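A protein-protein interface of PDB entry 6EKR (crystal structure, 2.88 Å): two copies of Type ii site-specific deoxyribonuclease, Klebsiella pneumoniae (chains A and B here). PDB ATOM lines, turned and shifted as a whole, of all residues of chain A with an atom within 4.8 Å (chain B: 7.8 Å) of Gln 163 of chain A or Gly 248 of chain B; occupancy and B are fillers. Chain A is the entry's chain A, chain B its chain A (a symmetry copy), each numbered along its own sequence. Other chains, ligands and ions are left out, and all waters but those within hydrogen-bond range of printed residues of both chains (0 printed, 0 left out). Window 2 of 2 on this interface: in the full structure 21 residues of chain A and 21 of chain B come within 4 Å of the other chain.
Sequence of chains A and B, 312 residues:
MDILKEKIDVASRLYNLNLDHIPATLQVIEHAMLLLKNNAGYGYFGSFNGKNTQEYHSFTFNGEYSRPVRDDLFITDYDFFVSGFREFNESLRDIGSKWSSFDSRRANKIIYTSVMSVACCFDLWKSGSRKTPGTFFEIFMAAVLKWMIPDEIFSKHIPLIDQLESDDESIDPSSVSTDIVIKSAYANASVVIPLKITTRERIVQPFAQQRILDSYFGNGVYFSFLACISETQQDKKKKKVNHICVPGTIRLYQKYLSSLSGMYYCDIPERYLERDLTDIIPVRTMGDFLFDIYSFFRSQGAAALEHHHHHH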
ATOM      1  N   PRO A 159      21.297 -23.355  15.229  1.00  0.00           N
ATOM      2  CA  PRO A 159      21.139 -22.331  16.271  1.00  0.00           C
ATOM      3  C   PRO A 159      20.098 -22.661  17.337  1.00  0.00           C
ATOM      4  O   PRO A 159      20.404 -22.611  18.529  1.00  0.00           O
ATOM      5  CB  PRO A 159      20.690 -21.086  15.482  1.00  0.00           C
ATOM      6  CG  PRO A 159      20.592 -21.533  14.016  1.00  0.00           C
ATOM      7  CD  PRO A 159      21.478 -22.731  13.909  1.00  0.00           C
ATOM      8  N   LEU A 160      18.883 -22.999  16.915  1.00  0.00           N
ATOM      9  CA  LEU A 160      17.796 -23.207  17.868  1.00  0.00           C
ATOM     10  C   LEU A 160      17.920 -24.512  18.664  1.00  0.00           C
ATOM     11  O   LEU A 160      17.461 -24.592  19.804  1.00  0.00           O
ATOM     12  CB  LEU A 160      16.435 -23.067  17.179  1.00  0.00           C
ATOM     13  CG  LEU A 160      15.901 -24.166  16.271  1.00  0.00           C
ATOM     14  CD1 LEU A 160      15.118 -25.166  17.110  1.00  0.00           C
ATOM     15  CD2 LEU A 160      15.020 -23.556  15.197  1.00  0.00           C
ATOM     16  N   ILE A 161      18.540 -25.524  18.058  1.00  0.00           N
ATOM     17  CA  ILE A 161      18.868 -26.767  18.762  1.00  0.00           C
ATOM     18  C   ILE A 161      20.008 -26.535  19.766  1.00  0.00           C
ATOM     19  O   ILE A 161      19.940 -27.020  20.899  1.00  0.00           O
ATOM     20  CB  ILE A 161      19.186 -27.939  17.783  1.00  0.00           C
ATOM     21  CG1 ILE A 161      17.910 -28.398  17.070  1.00  0.00           C
ATOM     22  CG2 ILE A 161      19.810 -29.127  18.520  1.00  0.00           C
ATOM     23  CD1 ILE A 161      18.150 -29.362  15.937  1.00  0.00           C
ATOM     24  N   ASP A 162      21.041 -25.788  19.359  1.00  0.00           N
ATOM     25  CA  ASP A 162      22.139 -25.412  20.264  1.00  0.00           C
ATOM     26  C   ASP A 162      21.640 -24.593  21.445  1.00  0.00           C
ATOM     27  O   ASP A 162      22.150 -24.723  22.558  1.00  0.00           O
ATOM     28  CB  ASP A 162      23.237 -24.645  19.522  1.00  0.00           C
ATOM     29  CG  ASP A 162      24.216 -25.561  18.825  1.00  0.00           C
ATOM     30  OD1 ASP A 162      24.260 -26.759  19.174  1.00  0.00           O
ATOM     31  OD2 ASP A 162      24.947 -25.094  17.929  1.00  0.00           O
ATOM     32  N   GLN A 163      20.637 -23.760  21.188  1.00  0.00           N
ATOM     33  CA  GLN A 163      20.028 -22.933  22.218  1.00  0.00           C
ATOM     34  C   GLN A 163      19.363 -23.784  23.303  1.00  0.00           C
ATOM     35  O   GLN A 163      19.590 -23.577  24.500  1.00  0.00           O
ATOM     36  CB  GLN A 163      19.023 -21.963  21.585  1.00  0.00           C
ATOM     37  CG  GLN A 163      18.575 -20.842  22.489  1.00  0.00           C
ATOM     38  CD  GLN A 163      19.714 -20.232  23.262  1.00  0.00           C
ATOM     39  OE1 GLN A 163      20.712 -19.799  22.690  1.00  0.00           O
ATOM     40  NE2 GLN A 163      19.574 -20.192  24.570  1.00  0.00           N
ATOM     41  N   LEU A 164      18.559 -24.749  22.867  1.00  0.00           N
ATOM     42  CA  LEU A 164      17.808 -25.609  23.771  1.00  0.00           C
ATOM     43  C   LEU A 164      18.724 -26.508  24.603  1.00  0.00           C
ATOM     44  O   LEU A 164      18.436 -26.787  25.769  1.00  0.00           O
ATOM     45  CB  LEU A 164      16.781 -26.442  22.989  1.00  0.00           C
ATOM     46  CG  LEU A 164      15.689 -25.688  22.214  1.00  0.00           C
ATOM     47  CD1 LEU A 164      15.087 -26.575  21.141  1.00  0.00           C
ATOM     48  CD2 LEU A 164      14.601 -25.140  23.122  1.00  0.00           C
ATOM     49  N   GLU A 165      19.829 -26.942  24.002  1.00  0.00           N
ATOM     50  CA  GLU A 165      20.773 -27.843  24.656  1.00  0.00           C
ATOM     51  C   GLU A 165      21.673 -27.095  25.632  1.00  0.00           C
ATOM     52  O   GLU A 165      22.015 -27.616  26.696  1.00  0.00           O
ATOM     53  CB  GLU A 165      21.597 -28.610  23.618  1.00  0.00           C
ATOM     54  CG  GLU A 165      20.760 -29.584  22.806  1.00  0.00           C
ATOM     55  CD  GLU A 165      21.553 -30.354  21.772  1.00  0.00           C
ATOM     56  OE1 GLU A 165      22.454 -29.767  21.142  1.00  0.00           O
ATOM     57  OE2 GLU A 165      21.256 -31.549  21.571  1.00  0.00           O
ATOM     58  N   SER A 166      22.046 -25.871  25.267  1.00  0.00           N
ATOM     59  CA  SER A 166      22.858 -25.020  26.130  1.00  0.00           C
ATOM     60  C   SER A 166      22.073 -24.624  27.373  1.00  0.00           C
ATOM     61  O   SER A 166      22.608 -24.655  28.481  1.00  0.00           O
ATOM     62  CB  SER A 166      23.332 -23.778  25.376  1.00  0.00           C
ATOM     63  OG  SER A 166      23.964 -22.855  26.241  1.00  0.00           O
ATOM     64  N   ASP A 167      20.803 -24.273  27.179  1.00  0.00           N
ATOM     65  CA  ASP A 167      19.925 -23.878  28.278  1.00  0.00           C
ATOM     66  C   ASP A 167      19.579 -25.044  29.202  1.00  0.00           C
ATOM     67  O   ASP A 167      19.446 -24.871  30.412  1.00  0.00           O
ATOM     68  CB  ASP A 167      18.647 -23.239  27.734  1.00  0.00           C
ATOM     69  CG  ASP A 167      18.811 -21.759  27.429  1.00  0.00           C
ATOM     70  OD1 ASP A 167      19.853 -21.163  27.770  1.00  0.00           O
ATOM     71  OD2 ASP A 167      17.878 -21.180  26.848  1.00  0.00           O
ATOM     72  N   CYS B 245      17.871 -18.846  34.861  1.00  0.00           N
ATOM     73  CA  CYS B 245      17.070 -18.319  33.767  1.00  0.00           C
ATOM     74  C   CYS B 245      17.483 -18.838  32.404  1.00  0.00           C
ATOM     75  O   CYS B 245      18.662 -19.076  32.125  1.00  0.00           O
ATOM     76  CB  CYS B 245      17.115 -16.799  33.764  1.00  0.00           C
ATOM     77  SG  CYS B 245      16.395 -16.087  35.218  1.00  0.00           S
ATOM     78  N   VAL B 246      16.486 -18.984  31.547  1.00  0.00           N
ATOM     79  CA  VAL B 246      16.689 -19.535  30.227  1.00  0.00           C
ATOM     80  C   VAL B 246      15.985 -18.627  29.188  1.00  0.00           C
ATOM     81  O   VAL B 246      15.046 -19.052  28.509  1.00  0.00           O
ATOM     82  CB  VAL B 246      16.246 -21.049  30.183  1.00  0.00           C
ATOM     83  CG1 VAL B 246      17.281 -21.926  30.837  1.00  0.00           C
ATOM     84  CG2 VAL B 246      14.915 -21.262  30.885  1.00  0.00           C
ATOM     85  N   PRO B 247      16.452 -17.367  29.055  1.00  0.00           N
ATOM     86  CA  PRO B 247      15.716 -16.371  28.275  1.00  0.00           C
ATOM     87  C   PRO B 247      15.581 -16.748  26.807  1.00  0.00           C
ATOM     88  O   PRO B 247      14.536 -16.494  26.211  1.00  0.00           O
ATOM     89  CB  PRO B 247      16.565 -15.103  28.426  1.00  0.00           C
ATOM     90  CG  PRO B 247      17.919 -15.582  28.782  1.00  0.00           C
ATOM     91  CD  PRO B 247      17.704 -16.810  29.599  1.00  0.00           C
ATOM     92  N   GLY B 248      16.626 -17.358  26.244  1.00  0.00           N
ATOM     93  CA  GLY B 248      16.600 -17.843  24.869  1.00  0.00           C
ATOM     94  C   GLY B 248      15.525 -18.893  24.669  1.00  0.00           C
ATOM     95  O   GLY B 248      14.773 -18.860  23.687  1.00  0.00           O
ATOM     96  N   THR B 249      15.442 -19.822  25.615  1.00  0.00           N
ATOM     97  CA  THR B 249      14.491 -20.915  25.538  1.00  0.00           C
ATOM     98  C   THR B 249      13.033 -20.439  25.578  1.00  0.00           C
ATOM     99  O   THR B 249      12.191 -20.922  24.815  1.00  0.00           O
ATOM    100  CB  THR B 249      14.807 -21.963  26.621  1.00  0.00           C
ATOM    101  OG1 THR B 249      15.870 -22.792  26.142  1.00  0.00           O
ATOM    102  CG2 THR B 249      13.609 -22.841  26.940  1.00  0.00           C
ATOM    103  N   ILE B 250      12.751 -19.472  26.442  1.00  0.00           N
ATOM    104  CA  ILE B 250      11.396 -18.970  26.612  1.00  0.00           C
ATOM    105  C   ILE B 250      10.952 -18.206  25.376  1.00  0.00           C
ATOM    106  O   ILE B 250       9.784 -18.252  24.999  1.00  0.00           O
ATOM    107  CB  ILE B 250      11.263 -18.108  27.883  1.00  0.00           C
ATOM    108  CG1 ILE B 250      11.672 -18.926  29.105  1.00  0.00           C
ATOM    109  CG2 ILE B 250       9.837 -17.647  28.069  1.00  0.00           C
ATOM    110  CD1 ILE B 250      11.835 -18.116  30.356  1.00  0.00           C
ATOM    111  N   ARG B 251      11.892 -17.520  24.737  1.00  0.00           N
ATOM    112  CA  ARG B 251      11.600 -16.815  23.495  1.00  0.00           C
ATOM    113  C   ARG B 251      11.282 -17.796  22.367  1.00  0.00           C
ATOM    114  O   ARG B 251      10.259 -17.666  21.693  1.00  0.00           O
ATOM    115  CB  ARG B 251      12.759 -15.906  23.103  1.00  0.00           C
ATOM    116  CG  ARG B 251      12.994 -14.722  24.033  1.00  0.00           C
ATOM    117  CD  ARG B 251      14.265 -13.995  23.636  1.00  0.00           C
ATOM    118  NE  ARG B 251      14.307 -13.766  22.195  1.00  0.00           N
ATOM    119  CZ  ARG B 251      15.363 -13.313  21.529  1.00  0.00           C
ATOM    120  NH1 ARG B 251      16.486 -13.019  22.174  1.00  0.00           N
ATOM    121  NH2 ARG B 251      15.294 -13.145  20.212  1.00  0.00           N
ATOM    122  N   LEU B 252      12.150 -18.788  22.173  1.00  0.00           N
ATOM    123  CA  LEU B 252      11.852 -19.884  21.259  1.00  0.00           C
ATOM    124  C   LEU B 252      10.487 -20.482  21.568  1.00  0.00           C
ATOM    125  O   LEU B 252       9.685 -20.713  20.660  1.00  0.00           O
ATOM    126  CB  LEU B 252      12.925 -20.968  21.321  1.00  0.00           C
ATOM    127  CG  LEU B 252      14.111 -20.883  20.355  1.00  0.00           C
ATOM    128  CD1 LEU B 252      15.002 -19.671  20.637  1.00  0.00           C
ATOM    129  CD2 LEU B 252      14.945 -22.158  20.427  1.00  0.00           C
ATOM    130  N   TYR B 253      10.209 -20.709  22.846  1.00  0.00           N
ATOM    131  CA  TYR B 253       8.936 -21.281  23.231  1.00  0.00           C
ATOM    132  C   TYR B 253       7.749 -20.372  22.915  1.00  0.00           C
ATOM    133  O   TYR B 253       6.789 -20.823  22.304  1.00  0.00           O
ATOM    134  CB  TYR B 253       8.946 -21.719  24.696  1.00  0.00           C
ATOM    135  CG  TYR B 253       9.778 -22.969  24.989  1.00  0.00           C
ATOM    136  CD1 TYR B 253      10.336 -23.736  23.964  1.00  0.00           C
ATOM    137  CD2 TYR B 253       9.980 -23.392  26.301  1.00  0.00           C
ATOM    138  CE1 TYR B 253      11.087 -24.867  24.244  1.00  0.00           C
ATOM    139  CE2 TYR B 253      10.720 -24.525  26.591  1.00  0.00           C
ATOM    140  CZ  TYR B 253      11.271 -25.259  25.564  1.00  0.00           C
ATOM    141  OH  TYR B 253      12.006 -26.385  25.876  1.00  0.00           O
ATOM    142  N   GLN B 254       7.829 -19.098  23.300  1.00  0.00           N
ATOM    143  CA  GLN B 254       6.773 -18.119  22.988  1.00  0.00           C
ATOM    144  C   GLN B 254       6.489 -17.974  21.504  1.00  0.00           C
ATOM    145  O   GLN B 254       5.329 -17.871  21.086  1.00  0.00           O
ATOM    146  CB  GLN B 254       7.115 -16.731  23.521  1.00  0.00           C
ATOM    147  CG  GLN B 254       6.494 -16.396  24.840  1.00  0.00           C
ATOM    148  CD  GLN B 254       4.998 -16.463  24.802  1.00  0.00           C
ATOM    149  OE1 GLN B 254       4.411 -17.494  25.111  1.00  0.00           O
ATOM    150  NE2 GLN B 254       4.369 -15.374  24.418  1.00  0.00           N
ATOM    151  N   TYR B 256       7.737 -19.994  18.712  1.00  0.00           N
ATOM    152  CA  TYR B 256       7.592 -21.134  17.819  1.00  0.00           C
ATOM    153  C   TYR B 256       6.847 -22.343  18.408  1.00  0.00           C
ATOM    154  O   TYR B 256       6.354 -23.185  17.661  1.00  0.00           O
ATOM    155  CB  TYR B 256       8.958 -21.531  17.247  1.00  0.00           C
ATOM    156  CG  TYR B 256       9.765 -20.352  16.724  1.00  0.00           C
ATOM    157  CD1 TYR B 256       9.445 -19.728  15.508  1.00  0.00           C
ATOM    158  CD2 TYR B 256      10.847 -19.859  17.445  1.00  0.00           C
ATOM    159  CE1 TYR B 256      10.189 -18.635  15.029  1.00  0.00           C
ATOM    160  CE2 TYR B 256      11.597 -18.775  16.987  1.00  0.00           C
ATOM    161  CZ  TYR B 256      11.270 -18.161  15.781  1.00  0.00           C
ATOM    162  OH  TYR B 256      12.035 -17.080  15.355  1.00  0.00           O
ATOM    163  N   ARG B 271      16.937 -10.936  35.316  1.00  0.00           N
ATOM    164  CA  ARG B 271      17.104 -11.227  33.889  1.00  0.00           C
ATOM    165  C   ARG B 271      15.789 -11.195  33.115  1.00  0.00           C
ATOM    166  O   ARG B 271      15.755 -10.745  31.976  1.00  0.00           O
ATOM    167  CB  ARG B 271      17.804 -12.573  33.675  1.00  0.00           C
ATOM    168  CG  ARG B 271      18.051 -12.970  32.204  1.00  0.00           C
ATOM    169  CD  ARG B 271      18.898 -11.944  31.454  1.00  0.00           C
ATOM    170  NE  ARG B 271      18.962 -12.194  30.013  1.00  0.00           N
ATOM    171  CZ  ARG B 271      18.082 -11.739  29.120  1.00  0.00           C
ATOM    172  NH1 ARG B 271      17.043 -11.012  29.504  1.00  0.00           N
ATOM    173  NH2 ARG B 271      18.231 -12.021  27.834  1.00  0.00           N
ATOM    174  N   TYR B 272      14.708 -11.664  33.731  1.00  0.00           N
ATOM    175  CA  TYR B 272      13.417 -11.718  33.053  1.00  0.00           C
ATOM    176  C   TYR B 272      12.713 -10.351  32.961  1.00  0.00           C
ATOM    177  O   TYR B 272      11.613 -10.258  32.411  1.00  0.00           O
ATOM    178  CB  TYR B 272      12.490 -12.779  33.678  1.00  0.00           C
ATOM    179  CG  TYR B 272      12.870 -14.230  33.404  1.00  0.00           C
ATOM    180  CD1 TYR B 272      13.846 -14.561  32.468  1.00  0.00           C
ATOM    181  CD2 TYR B 272      12.235 -15.274  34.072  1.00  0.00           C
ATOM    182  CE1 TYR B 272      14.187 -15.891  32.210  1.00  0.00           C
ATOM    183  CE2 TYR B 272      12.580 -16.611  33.829  1.00  0.00           C
ATOM    184  CZ  TYR B 272      13.556 -16.911  32.895  1.00  0.00           C
ATOM    185  OH  TYR B 272      13.899 -18.218  32.626  1.00  0.00           O
ATOM    186  N   ASP B 276      13.885  -8.221  25.772  1.00  0.00           N
ATOM    187  CA  ASP B 276      13.973  -9.435  24.943  1.00  0.00           C
ATOM    188  C   ASP B 276      12.933 -10.490  25.321  1.00  0.00           C
ATOM    189  O   ASP B 276      12.538 -11.289  24.479  1.00  0.00           O
ATOM    190  CB  ASP B 276      15.400 -10.020  24.888  1.00  0.00           C
ATOM    191  CG  ASP B 276      15.799 -10.815  26.147  1.00  0.00           C
ATOM    192  OD1 ASP B 276      15.529 -10.371  27.287  1.00  0.00           O
ATOM    193  OD2 ASP B 276      16.437 -11.884  25.987  1.00  0.00           O
ATOM    194  N   LEU B 277      12.481 -10.462  26.577  1.00  0.00           N
ATOM    195  CA  LEU B 277      11.352 -11.272  27.037  1.00  0.00           C
ATOM    196  C   LEU B 277      10.044 -10.497  27.114  1.00  0.00           C
ATOM    197  O   LEU B 277       9.008 -10.947  26.606  1.00  0.00           O
ATOM    198  CB  LEU B 277      11.636 -11.857  28.414  1.00  0.00           C
ATOM    199  CG  LEU B 277      12.115 -13.299  28.402  1.00  0.00           C
ATOM    200  CD1 LEU B 277      12.643 -13.631  29.751  1.00  0.00           C
ATOM    201  CD2 LEU B 277      10.986 -14.238  28.030  1.00  0.00           C
ATOM    202  N   ILE B 280       7.691  -9.881  24.109  1.00  0.00           N
ATOM    203  CA  ILE B 280       6.903 -10.970  23.540  1.00  0.00           C
ATOM    204  C   ILE B 280       6.054 -11.735  24.565  1.00  0.00           C
ATOM    205  O   ILE B 280       5.155 -12.473  24.171  1.00  0.00           O
ATOM    206  CB  ILE B 280       7.790 -11.941  22.736  1.00  0.00           C
ATOM    207  CG1 ILE B 280       8.796 -12.647  23.654  1.00  0.00           C
ATOM    208  CG2 ILE B 280       8.498 -11.198  21.593  1.00  0.00           C
ATOM    209  CD1 ILE B 280       9.405 -13.896  23.036  1.00  0.00           C
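OG1 of Thr 249 of chain B lies within hydrogen-bond range of OD2 of Asp 167 of chain A (2.7 Å).
The side-chain carboxylate (OD2) of Asp 167 of chain A lies within hydrogen-bond range of the side-chain amide nitrogen (NE2) of Gln 163 of chain A, 3.0 Å away.
N of Val 246 of chain B is in hydrogen-bond range of OH of Tyr 272 of chain B (2.9 Å).
Leu 252 of chain B touches Leu 160 of chain A.
CA of Gly 248 of chain B touches NE2 of Gln 163 of chain A, at 3.8 Å.
Tyr 253 of chain B touches Leu 164 of chain A (CE1 to CD2, 3.7 Å).
Val 246 of chain B touches Asp 167 of chain A (CG1 to CB, 3.6 Å).
Asp 167 of chain A touches Gly 248 of chain B.
Of the printed residues of chain B, Asp 167 of chain A touches Val 246 (3.6 Å), Gly 248 (3.9 Å) and Thr 249 (2.7 Å).
Of the printed residues of chain A, Val 246 of chain B touches Asp 167 (3.6 Å).
Printed residues of chain A within 4 Å of Gly 248 of chain B: Gln 163 (3.8 Å) and Asp 167 (3.9 Å).
Arg 251 of chain B touches none of the printed residues of chain A.
Of the printed residues of chain A, Leu 252 of chain B touches Leu 160 (3.6 Å).
The nearest residue of chain B that does not touch Gln 163 of chain A is Thr 249 of chain B (4.1 Å).
The nearest printed residue of chain B that does not touch Asp 167 of chain A is Pro 247 of chain B (4.6 Å).
Hydrophobic or aromatic side chains of chain B within 4 Å of the printed part of chain A: Val 246, Leu 252 and Tyr 253.
Printed residues of chain A that touch a printed residue of chain B: Leu 160, Gln 163, Leu 164 and Asp 167.
Hydrophobic or aromatic side chains of chain A that line the printed part of chain B: Leu 160 and Leu 164.
Among the printed residues, 6 pairs touch across the chains.
Among the printed residues, no Asp or Glu carboxylate lies within 4 Å of a Lys or Arg side-chain nitrogen of the other chain.
No position is printed for both chains.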
